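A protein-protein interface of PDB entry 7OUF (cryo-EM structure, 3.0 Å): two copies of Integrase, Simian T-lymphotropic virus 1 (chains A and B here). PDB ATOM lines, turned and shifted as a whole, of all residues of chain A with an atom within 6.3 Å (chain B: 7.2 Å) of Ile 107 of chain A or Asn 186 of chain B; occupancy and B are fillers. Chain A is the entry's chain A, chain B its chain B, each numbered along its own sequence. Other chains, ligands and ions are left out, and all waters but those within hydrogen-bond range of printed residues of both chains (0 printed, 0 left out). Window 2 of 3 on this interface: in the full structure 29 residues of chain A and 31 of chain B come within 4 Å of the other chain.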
ATOM      1  N   THR A 102     -12.474  -2.901  -9.614  1.00  0.00           N
ATOM      2  CA  THR A 102     -11.667  -1.730  -9.914  1.00  0.00           C
ATOM      3  C   THR A 102     -12.476  -0.792 -10.796  1.00  0.00           C
ATOM      4  O   THR A 102     -13.564  -1.130 -11.266  1.00  0.00           O
ATOM      5  CB  THR A 102     -10.349  -2.114 -10.595  1.00  0.00           C
ATOM      6  OG1 THR A 102      -9.519  -0.954 -10.723  1.00  0.00           O
ATOM      7  CG2 THR A 102     -10.614  -2.695 -11.973  1.00  0.00           C
ATOM      8  N   SER A 103     -11.929   0.405 -11.011  1.00  0.00           N
ATOM      9  CA  SER A 103     -12.602   1.379 -11.862  1.00  0.00           C
ATOM     10  C   SER A 103     -12.704   0.892 -13.300  1.00  0.00           C
ATOM     11  O   SER A 103     -13.691   1.188 -13.986  1.00  0.00           O
ATOM     12  CB  SER A 103     -11.872   2.718 -11.803  1.00  0.00           C
ATOM     13  OG  SER A 103     -12.557   3.701 -12.559  1.00  0.00           O
ATOM     14  N   SER A 104     -11.697   0.155 -13.776  1.00  0.00           N
ATOM     15  CA  SER A 104     -11.740  -0.363 -15.138  1.00  0.00           C
ATOM     16  C   SER A 104     -12.902  -1.328 -15.329  1.00  0.00           C
ATOM     17  O   SER A 104     -13.611  -1.268 -16.342  1.00  0.00           O
ATOM     18  CB  SER A 104     -10.414  -1.045 -15.478  1.00  0.00           C
ATOM     19  OG  SER A 104      -9.351  -0.111 -15.486  1.00  0.00           O
ATOM     20  N   GLU A 105     -13.119  -2.224 -14.366  1.00  0.00           N
ATOM     21  CA  GLU A 105     -14.227  -3.163 -14.491  1.00  0.00           C
ATOM     22  C   GLU A 105     -15.571  -2.471 -14.321  1.00  0.00           C
ATOM     23  O   GLU A 105     -16.557  -2.890 -14.932  1.00  0.00           O
ATOM     24  CB  GLU A 105     -14.076  -4.303 -13.489  1.00  0.00           C
ATOM     25  CG  GLU A 105     -12.893  -5.204 -13.781  1.00  0.00           C
ATOM     26  CD  GLU A 105     -12.774  -6.337 -12.792  1.00  0.00           C
ATOM     27  OE1 GLU A 105     -13.549  -6.346 -11.817  1.00  0.00           O
ATOM     28  OE2 GLU A 105     -11.912  -7.218 -12.990  1.00  0.00           O
ATOM     29  N   ALA A 106     -15.630  -1.413 -13.513  1.00  0.00           N
ATOM     30  CA  ALA A 106     -16.846  -0.610 -13.456  1.00  0.00           C
ATOM     31  C   ALA A 106     -17.145   0.017 -14.810  1.00  0.00           C
ATOM     32  O   ALA A 106     -18.297   0.021 -15.262  1.00  0.00           O
ATOM     33  CB  ALA A 106     -16.713   0.469 -12.382  1.00  0.00           C
ATOM     34  N   ILE A 107     -16.115   0.540 -15.478  1.00  0.00           N
ATOM     35  CA  ILE A 107     -16.295   1.110 -16.811  1.00  0.00           C
ATOM     36  C   ILE A 107     -16.779   0.046 -17.785  1.00  0.00           C
ATOM     37  O   ILE A 107     -17.694   0.281 -18.585  1.00  0.00           O
ATOM     38  CB  ILE A 107     -14.985   1.761 -17.290  1.00  0.00           C
ATOM     39  CG1 ILE A 107     -14.693   3.030 -16.489  1.00  0.00           C
ATOM     40  CG2 ILE A 107     -15.051   2.073 -18.774  1.00  0.00           C
ATOM     41  CD1 ILE A 107     -13.364   3.662 -16.822  1.00  0.00           C
ATOM     42  N   SER A 108     -16.168  -1.139 -17.737  1.00  0.00           N
ATOM     43  CA  SER A 108     -16.552  -2.211 -18.650  1.00  0.00           C
ATOM     44  C   SER A 108     -17.995  -2.641 -18.418  1.00  0.00           C
ATOM     45  O   SER A 108     -18.752  -2.858 -19.370  1.00  0.00           O
ATOM     46  CB  SER A 108     -15.607  -3.399 -18.492  1.00  0.00           C
ATOM     47  OG  SER A 108     -15.802  -4.035 -17.242  1.00  0.00           O
ATOM     48  N   SER A 109     -18.393  -2.771 -17.151  1.00  0.00           N
ATOM     49  CA  SER A 109     -19.764  -3.153 -16.836  1.00  0.00           C
ATOM     50  C   SER A 109     -20.753  -2.088 -17.287  1.00  0.00           C
ATOM     51  O   SER A 109     -21.826  -2.413 -17.806  1.00  0.00           O
ATOM     52  CB  SER A 109     -19.903  -3.411 -15.338  1.00  0.00           C
ATOM     53  OG  SER A 109     -18.938  -4.348 -14.896  1.00  0.00           O
ATOM     54  N   LEU A 110     -20.416  -0.812 -17.092  1.00  0.00           N
ATOM     55  CA  LEU A 110     -21.297   0.254 -17.553  1.00  0.00           C
ATOM     56  C   LEU A 110     -21.450   0.222 -19.067  1.00  0.00           C
ATOM     57  O   LEU A 110     -22.560   0.382 -19.588  1.00  0.00           O
ATOM     58  CB  LEU A 110     -20.768   1.612 -17.094  1.00  0.00           C
ATOM     59  CG  LEU A 110     -21.647   2.814 -17.440  1.00  0.00           C
ATOM     60  CD1 LEU A 110     -23.033   2.653 -16.850  1.00  0.00           C
ATOM     61  CD2 LEU A 110     -21.007   4.101 -16.961  1.00  0.00           C
ATOM     62  N   LEU A 111     -20.351   0.008 -19.792  1.00  0.00           N
ATOM     63  CA  LEU A 111     -20.435  -0.064 -21.247  1.00  0.00           C
ATOM     64  C   LEU A 111     -21.260  -1.265 -21.700  1.00  0.00           C
ATOM     65  O   LEU A 111     -22.049  -1.162 -22.646  1.00  0.00           O
ATOM     66  CB  LEU A 111     -19.033  -0.111 -21.851  1.00  0.00           C
ATOM     67  CG  LEU A 111     -18.230   1.185 -21.755  1.00  0.00           C
ATOM     68  CD1 LEU A 111     -16.898   1.036 -22.458  1.00  0.00           C
ATOM     69  CD2 LEU A 111     -19.016   2.349 -22.331  1.00  0.00           C
ATOM     70  N   HIS A 112     -21.090  -2.412 -21.040  1.00  0.00           N
ATOM     71  CA  HIS A 112     -21.886  -3.588 -21.373  1.00  0.00           C
ATOM     72  C   HIS A 112     -23.369  -3.338 -21.127  1.00  0.00           C
ATOM     73  O   HIS A 112     -24.221  -3.725 -21.939  1.00  0.00           O
ATOM     74  CB  HIS A 112     -21.399  -4.786 -20.557  1.00  0.00           C
ATOM     75  CG  HIS A 112     -21.785  -6.111 -21.131  1.00  0.00           C
ATOM     76  ND1 HIS A 112     -20.917  -6.884 -21.870  1.00  0.00           N
ATOM     77  CD2 HIS A 112     -22.944  -6.806 -21.067  1.00  0.00           C
ATOM     78  CE1 HIS A 112     -21.525  -7.996 -22.239  1.00  0.00           C
ATOM     79  NE2 HIS A 112     -22.757  -7.974 -21.765  1.00  0.00           N
ATOM     80  N   GLU A 135     -10.924   7.928 -13.316  1.00  0.00           N
ATOM     81  CA  GLU A 135     -11.231   7.105 -14.482  1.00  0.00           C
ATOM     82  C   GLU A 135     -12.734   7.036 -14.729  1.00  0.00           C
ATOM     83  O   GLU A 135     -13.202   7.277 -15.848  1.00  0.00           O
ATOM     84  CB  GLU A 135     -10.654   5.701 -14.299  1.00  0.00           C
ATOM     85  CG  GLU A 135      -9.155   5.664 -14.082  1.00  0.00           C
ATOM     86  CD  GLU A 135      -8.384   5.457 -15.371  1.00  0.00           C
ATOM     87  OE1 GLU A 135      -9.026   5.296 -16.431  1.00  0.00           O
ATOM     88  OE2 GLU A 135      -7.137   5.454 -15.326  1.00  0.00           O
ATOM     89  N   PHE A 136     -13.507   6.706 -13.692  1.00  0.00           N
ATOM     90  CA  PHE A 136     -14.954   6.608 -13.844  1.00  0.00           C
ATOM     91  C   PHE A 136     -15.572   7.965 -14.159  1.00  0.00           C
ATOM     92  O   PHE A 136     -16.511   8.056 -14.957  1.00  0.00           O
ATOM     93  CB  PHE A 136     -15.573   6.016 -12.580  1.00  0.00           C
ATOM     94  CG  PHE A 136     -16.953   5.461 -12.782  1.00  0.00           C
ATOM     95  CD1 PHE A 136     -18.068   6.269 -12.646  1.00  0.00           C
ATOM     96  CD2 PHE A 136     -17.136   4.131 -13.110  1.00  0.00           C
ATOM     97  CE1 PHE A 136     -19.336   5.760 -12.832  1.00  0.00           C
ATOM     98  CE2 PHE A 136     -18.401   3.616 -13.298  1.00  0.00           C
ATOM     99  CZ  PHE A 136     -19.503   4.434 -13.160  1.00  0.00           C
ATOM    100  N   ALA A 139     -14.908   8.663 -17.748  1.00  0.00           N
ATOM    101  CA  ALA A 139     -15.752   7.806 -18.572  1.00  0.00           C
ATOM    102  C   ALA A 139     -17.180   8.332 -18.633  1.00  0.00           C
ATOM    103  O   ALA A 139     -17.812   8.314 -19.695  1.00  0.00           O
ATOM    104  CB  ALA A 139     -15.729   6.377 -18.037  1.00  0.00           C
ATOM    105  N   HIS B  97     -16.762 -12.324 -27.450  1.00  0.00           N
ATOM    106  CA  HIS B  97     -15.361 -12.612 -27.720  1.00  0.00           C
ATOM    107  C   HIS B  97     -14.849 -13.692 -26.775  1.00  0.00           C
ATOM    108  O   HIS B  97     -15.142 -13.679 -25.578  1.00  0.00           O
ATOM    109  CB  HIS B  97     -14.507 -11.348 -27.598  1.00  0.00           C
ATOM    110  CG  HIS B  97     -14.273 -10.901 -26.188  1.00  0.00           C
ATOM    111  ND1 HIS B  97     -15.190 -10.153 -25.483  1.00  0.00           N
ATOM    112  CD2 HIS B  97     -13.223 -11.093 -25.356  1.00  0.00           C
ATOM    113  CE1 HIS B  97     -14.717  -9.905 -24.276  1.00  0.00           C
ATOM    114  NE2 HIS B  97     -13.525 -10.465 -24.172  1.00  0.00           N
ATOM    115  N   LEU B 172     -14.278  -1.984 -35.093  1.00  0.00           N
ATOM    116  CA  LEU B 172     -13.203  -2.270 -34.156  1.00  0.00           C
ATOM    117  C   LEU B 172     -11.911  -1.619 -34.617  1.00  0.00           C
ATOM    118  O   LEU B 172     -11.217  -0.971 -33.823  1.00  0.00           O
ATOM    119  CB  LEU B 172     -13.033  -3.781 -34.000  1.00  0.00           C
ATOM    120  CG  LEU B 172     -14.233  -4.499 -33.382  1.00  0.00           C
ATOM    121  CD1 LEU B 172     -14.151  -5.998 -33.606  1.00  0.00           C
ATOM    122  CD2 LEU B 172     -14.333  -4.180 -31.903  1.00  0.00           C
ATOM    123  N   TYR B 175     -11.979   1.908 -33.788  1.00  0.00           N
ATOM    124  CA  TYR B 175     -11.813   2.114 -32.356  1.00  0.00           C
ATOM    125  C   TYR B 175     -10.369   1.892 -31.939  1.00  0.00           C
ATOM    126  O   TYR B 175      -9.914   2.452 -30.935  1.00  0.00           O
ATOM    127  CB  TYR B 175     -12.751   1.191 -31.579  1.00  0.00           C
ATOM    128  CG  TYR B 175     -14.208   1.552 -31.735  1.00  0.00           C
ATOM    129  CD1 TYR B 175     -14.583   2.792 -32.222  1.00  0.00           C
ATOM    130  CD2 TYR B 175     -15.207   0.650 -31.404  1.00  0.00           C
ATOM    131  CE1 TYR B 175     -15.906   3.126 -32.373  1.00  0.00           C
ATOM    132  CE2 TYR B 175     -16.536   0.976 -31.552  1.00  0.00           C
ATOM    133  CZ  TYR B 175     -16.881   2.217 -32.036  1.00  0.00           C
ATOM    134  OH  TYR B 175     -18.204   2.555 -32.189  1.00  0.00           O
ATOM    135  N   LEU B 182      -7.163   0.643 -25.963  1.00  0.00           N
ATOM    136  CA  LEU B 182      -8.530   0.389 -25.523  1.00  0.00           C
ATOM    137  C   LEU B 182      -8.748  -1.108 -25.317  1.00  0.00           C
ATOM    138  O   LEU B 182      -8.349  -1.910 -26.170  1.00  0.00           O
ATOM    139  CB  LEU B 182      -9.518   0.942 -26.550  1.00  0.00           C
ATOM    140  CG  LEU B 182     -11.005   0.942 -26.201  1.00  0.00           C
ATOM    141  CD1 LEU B 182     -11.367   2.185 -25.416  1.00  0.00           C
ATOM    142  CD2 LEU B 182     -11.834   0.861 -27.468  1.00  0.00           C
ATOM    143  N   PRO B 183      -9.357  -1.522 -24.209  1.00  0.00           N
ATOM    144  CA  PRO B 183      -9.577  -2.955 -23.978  1.00  0.00           C
ATOM    145  C   PRO B 183     -10.573  -3.545 -24.964  1.00  0.00           C
ATOM    146  O   PRO B 183     -11.434  -2.851 -25.507  1.00  0.00           O
ATOM    147  CB  PRO B 183     -10.116  -3.007 -22.543  1.00  0.00           C
ATOM    148  CG  PRO B 183      -9.733  -1.699 -21.933  1.00  0.00           C
ATOM    149  CD  PRO B 183      -9.770  -0.711 -23.054  1.00  0.00           C
ATOM    150  N   MET B 184     -10.438  -4.854 -25.192  1.00  0.00           N
ATOM    151  CA  MET B 184     -11.265  -5.530 -26.187  1.00  0.00           C
ATOM    152  C   MET B 184     -12.740  -5.520 -25.799  1.00  0.00           C
ATOM    153  O   MET B 184     -13.609  -5.290 -26.650  1.00  0.00           O
ATOM    154  CB  MET B 184     -10.774  -6.964 -26.386  1.00  0.00           C
ATOM    155  CG  MET B 184     -11.581  -7.766 -27.392  1.00  0.00           C
ATOM    156  SD  MET B 184     -11.052  -7.493 -29.091  1.00  0.00           S
ATOM    157  CE  MET B 184     -12.616  -7.124 -29.879  1.00  0.00           C
ATOM    158  N   ASP B 185     -13.046  -5.781 -24.526  1.00  0.00           N
ATOM    159  CA  ASP B 185     -14.441  -5.821 -24.098  1.00  0.00           C
ATOM    160  C   ASP B 185     -15.109  -4.462 -24.255  1.00  0.00           C
ATOM    161  O   ASP B 185     -16.262  -4.373 -24.693  1.00  0.00           O
ATOM    162  CB  ASP B 185     -14.536  -6.306 -22.651  1.00  0.00           C
ATOM    163  CG  ASP B 185     -13.699  -5.473 -21.694  1.00  0.00           C
ATOM    164  OD1 ASP B 185     -12.962  -4.582 -22.160  1.00  0.00           O
ATOM    165  OD2 ASP B 185     -13.782  -5.709 -20.472  1.00  0.00           O
ATOM    166  N   ASN B 186     -14.396  -3.389 -23.901  1.00  0.00           N
ATOM    167  CA  ASN B 186     -14.937  -2.048 -24.083  1.00  0.00           C
ATOM    168  C   ASN B 186     -15.235  -1.775 -25.550  1.00  0.00           C
ATOM    169  O   ASN B 186     -16.308  -1.262 -25.891  1.00  0.00           O
ATOM    170  CB  ASN B 186     -13.951  -1.011 -23.544  1.00  0.00           C
ATOM    171  CG  ASN B 186     -13.912  -0.975 -22.034  1.00  0.00           C
ATOM    172  OD1 ASN B 186     -14.027  -2.006 -21.374  1.00  0.00           O
ATOM    173  ND2 ASN B 186     -13.738   0.216 -21.478  1.00  0.00           N
ATOM    174  N   ALA B 187     -14.293  -2.119 -26.431  1.00  0.00           N
ATOM    175  CA  ALA B 187     -14.492  -1.895 -27.856  1.00  0.00           C
ATOM    176  C   ALA B 187     -15.692  -2.672 -28.370  1.00  0.00           C
ATOM    177  O   ALA B 187     -16.506  -2.137 -29.127  1.00  0.00           O
ATOM    178  CB  ALA B 187     -13.233  -2.283 -28.628  1.00  0.00           C
ATOM    179  N   LEU B 188     -15.820  -3.938 -27.969  1.00  0.00           N
ATOM    180  CA  LEU B 188     -16.934  -4.749 -28.447  1.00  0.00           C
ATOM    181  C   LEU B 188     -18.268  -4.204 -27.955  1.00  0.00           C
ATOM    182  O   LEU B 188     -19.241  -4.152 -28.714  1.00  0.00           O
ATOM    183  CB  LEU B 188     -16.749  -6.203 -28.018  1.00  0.00           C
ATOM    184  CG  LEU B 188     -17.798  -7.186 -28.541  1.00  0.00           C
ATOM    185  CD1 LEU B 188     -17.830  -7.180 -30.057  1.00  0.00           C
ATOM    186  CD2 LEU B 188     -17.520  -8.582 -28.023  1.00  0.00           C
ATOM    187  N   SER B 189     -18.334  -3.784 -26.690  1.00  0.00           N
ATOM    188  CA  SER B 189     -19.583  -3.242 -26.165  1.00  0.00           C
ATOM    189  C   SER B 189     -19.963  -1.946 -26.872  1.00  0.00           C
ATOM    190  O   SER B 189     -21.128  -1.739 -27.232  1.00  0.00           O
ATOM    191  CB  SER B 189     -19.465  -3.023 -24.658  1.00  0.00           C
ATOM    192  OG  SER B 189     -19.128  -4.230 -23.999  1.00  0.00           O
ATOM    193  N   VAL B 190     -18.987  -1.061 -27.089  1.00  0.00           N
ATOM    194  CA  VAL B 190     -19.278   0.196 -27.771  1.00  0.00           C
ATOM    195  C   VAL B 190     -19.704  -0.060 -29.211  1.00  0.00           C
ATOM    196  O   VAL B 190     -20.624   0.587 -29.724  1.00  0.00           O
ATOM    197  CB  VAL B 190     -18.066   1.140 -27.691  1.00  0.00           C
ATOM    198  CG1 VAL B 190     -18.320   2.401 -28.498  1.00  0.00           C
ATOM    199  CG2 VAL B 190     -17.777   1.494 -26.247  1.00  0.00           C
ATOM    200  N   ALA B 191     -19.044  -1.004 -29.887  1.00  0.00           N
ATOM    201  CA  ALA B 191     -19.408  -1.322 -31.262  1.00  0.00           C
ATOM    202  C   ALA B 191     -20.808  -1.908 -31.345  1.00  0.00           C
ATOM    203  O   ALA B 191     -21.568  -1.575 -32.259  1.00  0.00           O
ATOM    204  CB  ALA B 191     -18.387  -2.285 -31.863  1.00  0.00           C
ATOM    205  N   LEU B 192     -21.167  -2.786 -30.406  1.00  0.00           N
ATOM    206  CA  LEU B 192     -22.519  -3.336 -30.394  1.00  0.00           C
ATOM    207  C   LEU B 192     -23.552  -2.246 -30.145  1.00  0.00           C
ATOM    208  O   LEU B 192     -24.604  -2.220 -30.795  1.00  0.00           O
ATOM    209  CB  LEU B 192     -22.630  -4.435 -29.341  1.00  0.00           C
ATOM    210  CG  LEU B 192     -21.961  -5.767 -29.680  1.00  0.00           C
ATOM    211  CD1 LEU B 192     -22.174  -6.768 -28.562  1.00  0.00           C
ATOM    212  CD2 LEU B 192     -22.476  -6.318 -31.000  1.00  0.00           C
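The backbone carbonyl oxygen of Glu 105 of chain A sits at hydrogen-bond distance from the side-chain hydroxyl of Ser 108 of chain A.
The side-chain carboxylate (OD1) of Asp 185 of chain B lies close to the side-chain amide oxygen (OD1) of Asn 186 of chain B (2.9 Å).
OG of Ser 189 of chain B sits at hydrogen-bond distance from O of Asp 185 of chain B.
Among the printed residues, merely in contact across the chains: Ile 107 of chain A with Asn 186 of chain B (3.5 Å), Ser 108 of chain A with Asp 185 of chain B (3.5 Å), Ser 108 of chain A with Asn 186 of chain B (3.6 Å), Leu 111 of chain A with Asn 186 of chain B (3.4 Å), Leu 111 of chain A with Ser 189 of chain B (3.8 Å), Leu 111 of chain A with Val 190 of chain B (3.9 Å) and His 112 of chain A with Ser 189 of chain B (3.8 Å).
Ser 103 of chain A touches none of the printed residues of chain B.
Ile 107 of chain A touches just one residue of chain B: Asn 186.
Printed residues of chain B within 4 Å of Ser 108 of chain A: Asp 185 and Asn 186.
Of the printed residues of chain B, Leu 111 of chain A touches Asn 186, Ser 189 and Val 190.
Of the printed residues of chain B, His 112 of chain A touches Ser 189.
Printed residues of chain A within 4 Å of Asp 185 of chain B: Ser 108 (3.5 Å).
Of chain A, only Ile 107 (3.5 Å), Ser 108 (3.6 Å) and Leu 111 (3.4 Å) come within 4 Å of Asn 186 of chain B.
Of the printed residues of chain A, Val 190 of chain B touches Leu 111 (3.9 Å).
The nearest residue of chain A that does not touch Asn 186 of chain B is Ser 104 of chain A (5.1 Å).
Hydrophobic or aromatic side chains of chain A within 4 Å of the printed part of chain B: Ile 107, Leu 111 and His 112.
Printed residues of chain B that touch a printed residue of chain A: Asp 185, Asn 186, Ser 189 and Val 190.
No position is printed for both chains.
Of the 7 pairs that touch across the chains among the printed residues, none has its exchanged pair printed and touching as well.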
